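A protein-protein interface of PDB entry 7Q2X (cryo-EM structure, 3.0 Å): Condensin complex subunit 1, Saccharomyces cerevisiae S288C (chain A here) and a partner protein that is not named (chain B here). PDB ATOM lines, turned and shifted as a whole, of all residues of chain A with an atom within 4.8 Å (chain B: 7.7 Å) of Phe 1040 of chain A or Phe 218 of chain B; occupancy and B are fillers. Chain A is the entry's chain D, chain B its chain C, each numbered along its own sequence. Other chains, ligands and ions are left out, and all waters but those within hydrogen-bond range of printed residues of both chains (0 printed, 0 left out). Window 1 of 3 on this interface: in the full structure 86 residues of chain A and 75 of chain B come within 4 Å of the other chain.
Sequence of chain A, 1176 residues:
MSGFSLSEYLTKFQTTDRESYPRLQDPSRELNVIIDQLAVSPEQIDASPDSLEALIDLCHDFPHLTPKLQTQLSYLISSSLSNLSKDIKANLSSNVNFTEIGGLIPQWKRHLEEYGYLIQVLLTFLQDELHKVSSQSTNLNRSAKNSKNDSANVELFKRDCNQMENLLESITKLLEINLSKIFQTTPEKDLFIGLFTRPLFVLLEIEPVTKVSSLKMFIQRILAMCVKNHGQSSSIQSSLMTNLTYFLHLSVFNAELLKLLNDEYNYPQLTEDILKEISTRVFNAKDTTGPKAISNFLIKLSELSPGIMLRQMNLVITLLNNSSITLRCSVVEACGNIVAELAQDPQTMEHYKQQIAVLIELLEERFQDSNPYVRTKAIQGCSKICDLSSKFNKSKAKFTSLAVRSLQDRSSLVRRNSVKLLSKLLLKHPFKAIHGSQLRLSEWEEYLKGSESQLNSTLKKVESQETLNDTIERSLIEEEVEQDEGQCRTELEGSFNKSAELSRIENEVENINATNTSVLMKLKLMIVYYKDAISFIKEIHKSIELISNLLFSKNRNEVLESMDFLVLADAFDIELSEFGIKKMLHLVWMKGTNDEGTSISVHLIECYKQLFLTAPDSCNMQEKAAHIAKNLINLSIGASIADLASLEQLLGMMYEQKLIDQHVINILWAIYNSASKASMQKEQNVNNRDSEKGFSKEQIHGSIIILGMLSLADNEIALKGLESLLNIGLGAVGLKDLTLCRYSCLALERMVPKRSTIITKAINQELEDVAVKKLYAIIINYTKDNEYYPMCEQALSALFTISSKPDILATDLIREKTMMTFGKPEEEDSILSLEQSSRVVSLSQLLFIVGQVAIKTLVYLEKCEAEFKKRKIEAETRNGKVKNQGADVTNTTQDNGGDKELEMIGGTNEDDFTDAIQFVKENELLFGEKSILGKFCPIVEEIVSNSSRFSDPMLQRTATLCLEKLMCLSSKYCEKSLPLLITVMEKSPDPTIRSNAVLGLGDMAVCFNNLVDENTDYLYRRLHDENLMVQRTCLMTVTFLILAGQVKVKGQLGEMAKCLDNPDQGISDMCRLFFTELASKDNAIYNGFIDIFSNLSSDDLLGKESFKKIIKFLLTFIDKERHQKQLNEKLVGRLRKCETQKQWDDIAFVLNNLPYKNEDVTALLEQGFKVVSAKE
O of Thr 1033 of chain A is in hydrogen-bond range of OG1 of Thr 1037 of chain A (2.8 Å).
Val 216 of chain B touches Leu 999 of chain A (CB to CD1, 3.6 Å).
Leu 999 of chain A touches Phe 218 of chain B (CD2 to CD2, 3.5 Å).
CB of Met 1036 of chain A touches CE2 of Phe 218 of chain B, at 3.5 Å.
Phe 218 of chain B touches Thr 1037 of chain A (CE2 to OG1, 3.4 Å).
Phe 1040 of chain A touches Ala 191 of chain B (CZ to CB, 3.8 Å).
CD1 of Phe 1040 of chain A touches CD1 of Leu 192 of chain B, at 3.5 Å.
Phe 195 of chain B touches Phe 1040 of chain A.
Phe 1040 of chain A touches Phe 218 of chain B.
Leu 1043 of chain A touches Leu 192 of chain B.
CB of Ala 1044 of chain A touches CE2 of Phe 195 of chain B, 3.5 Å away.
Of the printed residues of chain B, Leu 999 of chain A touches Leu 204 (3.7 Å), Val 216 (3.6 Å) and Phe 218 (3.5 Å).
Val 1038 of chain A touches none of the printed residues of chain B.
Phe 1040 of chain A touches just these residues of chain B: Phe 188, Ala 191, Leu 192, Phe 195 and Phe 218.
Printed residues of chain A within 4 Å of Phe 195 of chain B: Phe 1040 and Ala 1044.
Printed residues of chain A within 4 Å of Asp 196 of chain B: Ala 1044 (3.9 Å).
Of the printed residues of chain A, Leu 204 of chain B touches Leu 999 (3.7 Å).
Phe 218 of chain B touches just these residues of chain A: Leu 999, Met 1036, Thr 1037 and Phe 1040.
Printed residues of chain A within 4 Å of Ala 220 of chain B: Met 1036 (3.7 Å).
The nearest residue of chain A that does not touch Phe 218 of chain B is Thr 1033 of chain A (4.1 Å).
The nearest printed residue of chain A that does not touch Ala 220 of chain B is Phe 1040 of chain A (4.9 Å).
Among the printed residues, no Asp or Glu carboxylate lies within 4 Å of a Lys or Arg side-chain nitrogen of the other chain.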
ATOM      1  N   LEU A 999      11.112  -9.678 -21.581  1.00  0.00           N
ATOM      2  CA  LEU A 999       9.710  -9.826 -21.958  1.00  0.00           C
ATOM      3  C   LEU A 999       9.119 -11.114 -21.397  1.00  0.00           C
ATOM      4  O   LEU A 999       7.979 -11.127 -20.917  1.00  0.00           O
ATOM      5  CB  LEU A 999       9.570  -9.793 -23.479  1.00  0.00           C
ATOM      6  CG  LEU A 999       9.832  -8.445 -24.151  1.00  0.00           C
ATOM      7  CD1 LEU A 999       9.918  -8.607 -25.657  1.00  0.00           C
ATOM      8  CD2 LEU A 999       8.751  -7.449 -23.777  1.00  0.00           C
ATOM      9  N   THR A1033      13.260  -1.606 -22.987  1.00  0.00           N
ATOM     10  CA  THR A1033      12.293  -2.697 -22.906  1.00  0.00           C
ATOM     11  C   THR A1033      12.008  -3.073 -21.457  1.00  0.00           C
ATOM     12  O   THR A1033      10.852  -3.318 -21.085  1.00  0.00           O
ATOM     13  CB  THR A1033      12.797  -3.912 -23.685  1.00  0.00           C
ATOM     14  OG1 THR A1033      14.123  -4.242 -23.256  1.00  0.00           O
ATOM     15  CG2 THR A1033      12.807  -3.621 -25.177  1.00  0.00           C
ATOM     16  N   MET A1036       9.772  -0.394 -19.918  1.00  0.00           N
ATOM     17  CA  MET A1036       8.391  -0.520 -20.381  1.00  0.00           C
ATOM     18  C   MET A1036       7.684  -1.694 -19.710  1.00  0.00           C
ATOM     19  O   MET A1036       6.527  -1.574 -19.282  1.00  0.00           O
ATOM     20  CB  MET A1036       8.358  -0.668 -21.902  1.00  0.00           C
ATOM     21  CG  MET A1036       8.534   0.635 -22.660  1.00  0.00           C
ATOM     22  SD  MET A1036       6.981   1.527 -22.857  1.00  0.00           S
ATOM     23  CE  MET A1036       6.040   0.355 -23.830  1.00  0.00           C
ATOM     24  N   THR A1037       8.365  -2.840 -19.610  1.00  0.00           N
ATOM     25  CA  THR A1037       7.766  -4.000 -18.957  1.00  0.00           C
ATOM     26  C   THR A1037       7.489  -3.725 -17.484  1.00  0.00           C
ATOM     27  O   THR A1037       6.424  -4.085 -16.966  1.00  0.00           O
ATOM     28  CB  THR A1037       8.676  -5.219 -19.112  1.00  0.00           C
ATOM     29  OG1 THR A1037       9.058  -5.358 -20.486  1.00  0.00           O
ATOM     30  CG2 THR A1037       7.955  -6.480 -18.664  1.00  0.00           C
ATOM     31  N   VAL A1038       8.436  -3.084 -16.794  1.00  0.00           N
ATOM     32  CA  VAL A1038       8.246  -2.760 -15.383  1.00  0.00           C
ATOM     33  C   VAL A1038       7.096  -1.776 -15.215  1.00  0.00           C
ATOM     34  O   VAL A1038       6.304  -1.879 -14.272  1.00  0.00           O
ATOM     35  CB  VAL A1038       9.559  -2.220 -14.783  1.00  0.00           C
ATOM     36  CG1 VAL A1038       9.295  -1.460 -13.493  1.00  0.00           C
ATOM     37  CG2 VAL A1038      10.537  -3.360 -14.541  1.00  0.00           C
ATOM     38  N   THR A1039       6.983  -0.809 -16.129  1.00  0.00           N
ATOM     39  CA  THR A1039       5.889   0.153 -16.062  1.00  0.00           C
ATOM     40  C   THR A1039       4.540  -0.532 -16.223  1.00  0.00           C
ATOM     41  O   THR A1039       3.605  -0.256 -15.462  1.00  0.00           O
ATOM     42  CB  THR A1039       6.070   1.231 -17.131  1.00  0.00           C
ATOM     43  OG1 THR A1039       7.441   1.648 -17.165  1.00  0.00           O
ATOM     44  CG2 THR A1039       5.187   2.431 -16.829  1.00  0.00           C
ATOM     45  N   PHE A1040       4.417  -1.429 -17.204  1.00  0.00           N
ATOM     46  CA  PHE A1040       3.156  -2.147 -17.369  1.00  0.00           C
ATOM     47  C   PHE A1040       2.850  -3.019 -16.156  1.00  0.00           C
ATOM     48  O   PHE A1040       1.703  -3.073 -15.695  1.00  0.00           O
ATOM     49  CB  PHE A1040       3.171  -2.986 -18.646  1.00  0.00           C
ATOM     50  CG  PHE A1040       2.915  -2.192 -19.894  1.00  0.00           C
ATOM     51  CD1 PHE A1040       2.450  -0.890 -19.819  1.00  0.00           C
ATOM     52  CD2 PHE A1040       3.103  -2.757 -21.143  1.00  0.00           C
ATOM     53  CE1 PHE A1040       2.203  -0.160 -20.965  1.00  0.00           C
ATOM     54  CE2 PHE A1040       2.856  -2.031 -22.292  1.00  0.00           C
ATOM     55  CZ  PHE A1040       2.406  -0.731 -22.202  1.00  0.00           C
ATOM     56  N   LEU A1041       3.865  -3.703 -15.618  1.00  0.00           N
ATOM     57  CA  LEU A1041       3.642  -4.557 -14.454  1.00  0.00           C
ATOM     58  C   LEU A1041       3.196  -3.744 -13.245  1.00  0.00           C
ATOM     59  O   LEU A1041       2.309  -4.168 -12.495  1.00  0.00           O
ATOM     60  CB  LEU A1041       4.910  -5.347 -14.133  1.00  0.00           C
ATOM     61  CG  LEU A1041       5.186  -6.569 -15.012  1.00  0.00           C
ATOM     62  CD1 LEU A1041       6.561  -7.145 -14.714  1.00  0.00           C
ATOM     63  CD2 LEU A1041       4.106  -7.621 -14.821  1.00  0.00           C
ATOM     64  N   ILE A1042       3.801  -2.573 -13.037  1.00  0.00           N
ATOM     65  CA  ILE A1042       3.451  -1.743 -11.888  1.00  0.00           C
ATOM     66  C   ILE A1042       2.057  -1.152 -12.061  1.00  0.00           C
ATOM     67  O   ILE A1042       1.242  -1.161 -11.129  1.00  0.00           O
ATOM     68  CB  ILE A1042       4.511  -0.646 -11.681  1.00  0.00           C
ATOM     69  CG1 ILE A1042       5.736  -1.217 -10.965  1.00  0.00           C
ATOM     70  CG2 ILE A1042       3.933   0.525 -10.900  1.00  0.00           C
ATOM     71  CD1 ILE A1042       6.923  -0.283 -10.950  1.00  0.00           C
ATOM     72  N   LEU A1043       1.756  -0.638 -13.256  1.00  0.00           N
ATOM     73  CA  LEU A1043       0.457  -0.016 -13.485  1.00  0.00           C
ATOM     74  C   LEU A1043      -0.674  -1.034 -13.431  1.00  0.00           C
ATOM     75  O   LEU A1043      -1.783  -0.701 -12.996  1.00  0.00           O
ATOM     76  CB  LEU A1043       0.457   0.717 -14.825  1.00  0.00           C
ATOM     77  CG  LEU A1043       1.349   1.960 -14.890  1.00  0.00           C
ATOM     78  CD1 LEU A1043       1.404   2.519 -16.303  1.00  0.00           C
ATOM     79  CD2 LEU A1043       0.875   3.019 -13.907  1.00  0.00           C
ATOM     80  N   ALA A1044      -0.422  -2.272 -13.862  1.00  0.00           N
ATOM     81  CA  ALA A1044      -1.437  -3.311 -13.752  1.00  0.00           C
ATOM     82  C   ALA A1044      -1.596  -3.831 -12.330  1.00  0.00           C
ATOM     83  O   ALA A1044      -2.558  -4.557 -12.060  1.00  0.00           O
ATOM     84  CB  ALA A1044      -1.107  -4.472 -14.690  1.00  0.00           C
ATOM     85  N   LEU B 187      -1.537   5.960 -27.618  1.00  0.00           N
ATOM     86  CA  LEU B 187      -1.097   4.603 -27.926  1.00  0.00           C
ATOM     87  C   LEU B 187      -0.645   3.868 -26.671  1.00  0.00           C
ATOM     88  O   LEU B 187      -0.906   2.670 -26.518  1.00  0.00           O
ATOM     89  CB  LEU B 187       0.019   4.637 -28.968  1.00  0.00           C
ATOM     90  CG  LEU B 187      -0.428   5.064 -30.366  1.00  0.00           C
ATOM     91  CD1 LEU B 187       0.767   5.244 -31.277  1.00  0.00           C
ATOM     92  CD2 LEU B 187      -1.402   4.053 -30.948  1.00  0.00           C
ATOM     93  N   PHE B 188       0.036   4.571 -25.761  1.00  0.00           N
ATOM     94  CA  PHE B 188       0.398   3.963 -24.485  1.00  0.00           C
ATOM     95  C   PHE B 188      -0.845   3.590 -23.688  1.00  0.00           C
ATOM     96  O   PHE B 188      -0.885   2.534 -23.047  1.00  0.00           O
ATOM     97  CB  PHE B 188       1.287   4.913 -23.683  1.00  0.00           C
ATOM     98  CG  PHE B 188       1.866   4.300 -22.440  1.00  0.00           C
ATOM     99  CD1 PHE B 188       3.041   3.571 -22.494  1.00  0.00           C
ATOM    100  CD2 PHE B 188       1.238   4.458 -21.216  1.00  0.00           C
ATOM    101  CE1 PHE B 188       3.577   3.008 -21.352  1.00  0.00           C
ATOM    102  CE2 PHE B 188       1.769   3.896 -20.071  1.00  0.00           C
ATOM    103  CZ  PHE B 188       2.940   3.170 -20.140  1.00  0.00           C
ATOM    104  N   LYS B 189      -1.870   4.446 -23.717  1.00  0.00           N
ATOM    105  CA  LYS B 189      -3.121   4.132 -23.033  1.00  0.00           C
ATOM    106  C   LYS B 189      -3.783   2.896 -23.630  1.00  0.00           C
ATOM    107  O   LYS B 189      -4.283   2.033 -22.897  1.00  0.00           O
ATOM    108  CB  LYS B 189      -4.062   5.335 -23.100  1.00  0.00           C
ATOM    109  CG  LYS B 189      -5.369   5.160 -22.347  1.00  0.00           C
ATOM    110  CD  LYS B 189      -6.211   6.425 -22.428  1.00  0.00           C
ATOM    111  CE  LYS B 189      -7.481   6.305 -21.605  1.00  0.00           C
ATOM    112  NZ  LYS B 189      -8.417   5.296 -22.172  1.00  0.00           N
ATOM    113  N   LYS B 190      -3.800   2.795 -24.961  1.00  0.00           N
ATOM    114  CA  LYS B 190      -4.382   1.623 -25.611  1.00  0.00           C
ATOM    115  C   LYS B 190      -3.610   0.356 -25.262  1.00  0.00           C
ATOM    116  O   LYS B 190      -4.210  -0.692 -24.988  1.00  0.00           O
ATOM    117  CB  LYS B 190      -4.419   1.830 -27.125  1.00  0.00           C
ATOM    118  CG  LYS B 190      -5.081   0.701 -27.893  1.00  0.00           C
ATOM    119  CD  LYS B 190      -5.215   1.046 -29.366  1.00  0.00           C
ATOM    120  CE  LYS B 190      -4.126   0.378 -30.190  1.00  0.00           C
ATOM    121  NZ  LYS B 190      -4.676  -0.279 -31.407  1.00  0.00           N
ATOM    122  N   ALA B 191      -2.277   0.434 -25.273  1.00  0.00           N
ATOM    123  CA  ALA B 191      -1.464  -0.722 -24.906  1.00  0.00           C
ATOM    124  C   ALA B 191      -1.703  -1.123 -23.458  1.00  0.00           C
ATOM    125  O   ALA B 191      -1.780  -2.315 -23.141  1.00  0.00           O
ATOM    126  CB  ALA B 191       0.015  -0.422 -25.146  1.00  0.00           C
ATOM    127  N   LEU B 192      -1.823  -0.139 -22.563  1.00  0.00           N
ATOM    128  CA  LEU B 192      -2.103  -0.432 -21.161  1.00  0.00           C
ATOM    129  C   LEU B 192      -3.462  -1.097 -20.995  1.00  0.00           C
ATOM    130  O   LEU B 192      -3.608  -2.038 -20.207  1.00  0.00           O
ATOM    131  CB  LEU B 192      -2.029   0.854 -20.339  1.00  0.00           C
ATOM    132  CG  LEU B 192      -1.896   0.718 -18.823  1.00  0.00           C
ATOM    133  CD1 LEU B 192      -0.744  -0.203 -18.459  1.00  0.00           C
ATOM    134  CD2 LEU B 192      -1.707   2.089 -18.196  1.00  0.00           C
ATOM    135  N   VAL B 193      -4.472  -0.620 -21.726  1.00  0.00           N
ATOM    136  CA  VAL B 193      -5.803  -1.221 -21.644  1.00  0.00           C
ATOM    137  C   VAL B 193      -5.763  -2.663 -22.139  1.00  0.00           C
ATOM    138  O   VAL B 193      -6.321  -3.573 -21.511  1.00  0.00           O
ATOM    139  CB  VAL B 193      -6.821  -0.378 -22.433  1.00  0.00           C
ATOM    140  CG1 VAL B 193      -8.092  -1.174 -22.689  1.00  0.00           C
ATOM    141  CG2 VAL B 193      -7.135   0.909 -21.686  1.00  0.00           C
ATOM    142  N   PHE B 195      -3.171  -4.660 -22.218  1.00  0.00           N
ATOM    143  CA  PHE B 195      -2.421  -5.449 -21.248  1.00  0.00           C
ATOM    144  C   PHE B 195      -3.264  -5.771 -20.021  1.00  0.00           C
ATOM    145  O   PHE B 195      -3.207  -6.888 -19.494  1.00  0.00           O
ATOM    146  CB  PHE B 195      -1.150  -4.695 -20.856  1.00  0.00           C
ATOM    147  CG  PHE B 195      -0.302  -5.410 -19.848  1.00  0.00           C
ATOM    148  CD1 PHE B 195       0.551  -6.427 -20.238  1.00  0.00           C
ATOM    149  CD2 PHE B 195      -0.343  -5.051 -18.513  1.00  0.00           C
ATOM    150  CE1 PHE B 195       1.338  -7.079 -19.311  1.00  0.00           C
ATOM    151  CE2 PHE B 195       0.441  -5.699 -17.584  1.00  0.00           C
ATOM    152  CZ  PHE B 195       1.282  -6.712 -17.984  1.00  0.00           C
ATOM    153  N   ASP B 196      -4.055  -4.805 -19.551  1.00  0.00           N
ATOM    154  CA  ASP B 196      -4.888  -5.013 -18.375  1.00  0.00           C
ATOM    155  C   ASP B 196      -6.164  -5.784 -18.684  1.00  0.00           C
ATOM    156  O   ASP B 196      -6.909  -6.111 -17.754  1.00  0.00           O
ATOM    157  CB  ASP B 196      -5.248  -3.671 -17.735  1.00  0.00           C
ATOM    158  CG  ASP B 196      -5.400  -3.768 -16.231  1.00  0.00           C
ATOM    159  OD1 ASP B 196      -4.885  -4.741 -15.642  1.00  0.00           O
ATOM    160  OD2 ASP B 196      -6.043  -2.877 -15.637  1.00  0.00           O
ATOM    161  N   LEU B 204       1.823 -10.409 -24.082  1.00  0.00           N
ATOM    162  CA  LEU B 204       2.970  -9.581 -24.443  1.00  0.00           C
ATOM    163  C   LEU B 204       3.863 -10.252 -25.480  1.00  0.00           C
ATOM    164  O   LEU B 204       4.847  -9.646 -25.921  1.00  0.00           O
ATOM    165  CB  LEU B 204       3.806  -9.185 -23.215  1.00  0.00           C
ATOM    166  CG  LEU B 204       4.740  -7.975 -23.305  1.00  0.00           C
ATOM    167  CD1 LEU B 204       3.943  -6.710 -23.576  1.00  0.00           C
ATOM    168  CD2 LEU B 204       5.548  -7.836 -22.026  1.00  0.00           C
ATOM    169  N   THR B 207       0.554 -10.054 -29.006  1.00  0.00           N
ATOM    170  CA  THR B 207       0.176  -8.729 -29.488  1.00  0.00           C
ATOM    171  C   THR B 207       1.342  -8.035 -30.180  1.00  0.00           C
ATOM    172  O   THR B 207       1.167  -7.410 -31.232  1.00  0.00           O
ATOM    173  CB  THR B 207      -0.341  -7.877 -28.330  1.00  0.00           C
ATOM    174  OG1 THR B 207       0.763  -7.446 -27.522  1.00  0.00           O
ATOM    175  CG2 THR B 207      -1.307  -8.678 -27.471  1.00  0.00           C
ATOM    176  N   LEU B 208       2.538  -8.130 -29.604  1.00  0.00           N
ATOM    177  CA  LEU B 208       3.700  -7.478 -30.190  1.00  0.00           C
ATOM    178  C   LEU B 208       4.194  -8.242 -31.413  1.00  0.00           C
ATOM    179  O   LEU B 208       4.011  -9.457 -31.535  1.00  0.00           O
ATOM    180  CB  LEU B 208       4.824  -7.363 -29.161  1.00  0.00           C
ATOM    181  CG  LEU B 208       4.501  -6.640 -27.853  1.00  0.00           C
ATOM    182  CD1 LEU B 208       5.701  -6.679 -26.921  1.00  0.00           C
ATOM    183  CD2 LEU B 208       4.071  -5.208 -28.120  1.00  0.00           C
ATOM    184  N   ASN B 209       4.827  -7.512 -32.325  1.00  0.00           N
ATOM    185  CA  ASN B 209       5.410  -8.097 -33.519  1.00  0.00           C
ATOM    186  C   ASN B 209       6.892  -8.389 -33.296  1.00  0.00           C
ATOM    187  O   ASN B 209       7.485  -8.004 -32.287  1.00  0.00           O
ATOM    188  CB  ASN B 209       5.220  -7.167 -34.719  1.00  0.00           C
ATOM    189  CG  ASN B 209       3.778  -6.743 -34.902  1.00  0.00           C
ATOM    190  OD1 ASN B 209       2.874  -7.277 -34.260  1.00  0.00           O
ATOM    191  ND2 ASN B 209       3.554  -5.774 -35.782  1.00  0.00           N
ATOM    192  N   ARG B 215      13.803 -10.081 -32.925  1.00  0.00           N
ATOM    193  CA  ARG B 215      13.602  -9.206 -31.780  1.00  0.00           C
ATOM    194  C   ARG B 215      12.138  -8.801 -31.713  1.00  0.00           C
ATOM    195  O   ARG B 215      11.571  -8.348 -32.712  1.00  0.00           O
ATOM    196  CB  ARG B 215      14.490  -7.964 -31.872  1.00  0.00           C
ATOM    197  CG  ARG B 215      14.354  -7.021 -30.690  1.00  0.00           C
ATOM    198  CD  ARG B 215      15.527  -6.060 -30.614  1.00  0.00           C
ATOM    199  NE  ARG B 215      15.267  -4.813 -31.323  1.00  0.00           N
ATOM    200  CZ  ARG B 215      14.485  -3.842 -30.871  1.00  0.00           C
ATOM    201  NH1 ARG B 215      13.870  -3.935 -29.703  1.00  0.00           N
ATOM    202  NH2 ARG B 215      14.319  -2.748 -31.607  1.00  0.00           N
ATOM    203  N   VAL B 216      11.536  -8.961 -30.539  1.00  0.00           N
ATOM    204  CA  VAL B 216      10.139  -8.592 -30.335  1.00  0.00           C
ATOM    205  C   VAL B 216      10.088  -7.093 -30.060  1.00  0.00           C
ATOM    206  O   VAL B 216      10.610  -6.618 -29.049  1.00  0.00           O
ATOM    207  CB  VAL B 216       9.509  -9.391 -29.188  1.00  0.00           C
ATOM    208  CG1 VAL B 216       8.040  -9.041 -29.045  1.00  0.00           C
ATOM    209  CG2 VAL B 216       9.687 -10.882 -29.423  1.00  0.00           C
ATOM    210  N   ILE B 217       9.457  -6.344 -30.964  1.00  0.00           N
ATOM    211  CA  ILE B 217       9.401  -4.895 -30.826  1.00  0.00           C
ATOM    212  C   ILE B 217       8.409  -4.531 -29.731  1.00  0.00           C
ATOM    213  O   ILE B 217       7.235  -4.921 -29.776  1.00  0.00           O
ATOM    214  CB  ILE B 217       9.022  -4.239 -32.162  1.00  0.00           C
ATOM    215  CG1 ILE B 217      10.081  -4.539 -33.226  1.00  0.00           C
ATOM    216  CG2 ILE B 217       8.847  -2.738 -31.989  1.00  0.00           C
ATOM    217  CD1 ILE B 217      11.504  -4.348 -32.749  1.00  0.00           C
ATOM    218  N   PHE B 218       8.879  -3.776 -28.738  1.00  0.00           N
ATOM    219  CA  PHE B 218       8.065  -3.359 -27.596  1.00  0.00           C
ATOM    220  C   PHE B 218       8.245  -1.854 -27.425  1.00  0.00           C
ATOM    221  O   PHE B 218       9.120  -1.404 -26.680  1.00  0.00           O
ATOM    222  CB  PHE B 218       8.459  -4.125 -26.338  1.00  0.00           C
ATOM    223  CG  PHE B 218       7.541  -3.893 -25.174  1.00  0.00           C
ATOM    224  CD1 PHE B 218       6.215  -3.549 -25.375  1.00  0.00           C
ATOM    225  CD2 PHE B 218       8.003  -4.027 -23.876  1.00  0.00           C
ATOM    226  CE1 PHE B 218       5.371  -3.338 -24.306  1.00  0.00           C
ATOM    227  CE2 PHE B 218       7.162  -3.821 -22.803  1.00  0.00           C
ATOM    228  CZ  PHE B 218       5.846  -3.475 -23.018  1.00  0.00           C
ATOM    229  N   ASP B 219       7.415  -1.078 -28.119  1.00  0.00           N
ATOM    230  CA  ASP B 219       7.467   0.377 -28.023  1.00  0.00           C
ATOM    231  C   ASP B 219       6.067   0.917 -28.261  1.00  0.00           C
ATOM    232  O   ASP B 219       5.471   0.654 -29.309  1.00  0.00           O
ATOM    233  CB  ASP B 219       8.456   0.962 -29.035  1.00  0.00           C
ATOM    234  CG  ASP B 219       8.697   2.449 -28.830  1.00  0.00           C
ATOM    235  OD1 ASP B 219       8.077   3.043 -27.923  1.00  0.00           O
ATOM    236  OD2 ASP B 219       9.512   3.025 -29.579  1.00  0.00           O
ATOM    237  N   ALA B 220       5.547   1.668 -27.291  1.00  0.00           N
ATOM    238  CA  ALA B 220       4.219   2.277 -27.372  1.00  0.00           C
ATOM    239  C   ALA B 220       4.372   3.759 -27.044  1.00  0.00           C
ATOM    240  O   ALA B 220       4.210   4.169 -25.892  1.00  0.00           O
ATOM    241  CB  ALA B 220       3.235   1.585 -26.434  1.00  0.00           C
ATOM    242  N   SER B 221       4.684   4.558 -28.061  1.00  0.00           N
ATOM    243  CA  SER B 221       4.877   5.989 -27.878  1.00  0.00           C
ATOM    244  C   SER B 221       4.677   6.684 -29.216  1.00  0.00           C
ATOM    245  O   SER B 221       4.700   6.051 -30.274  1.00  0.00           O
ATOM    246  CB  SER B 221       6.265   6.301 -27.308  1.00  0.00           C
ATOM    247  OG  SER B 221       7.286   5.936 -28.222  1.00  0.00           O
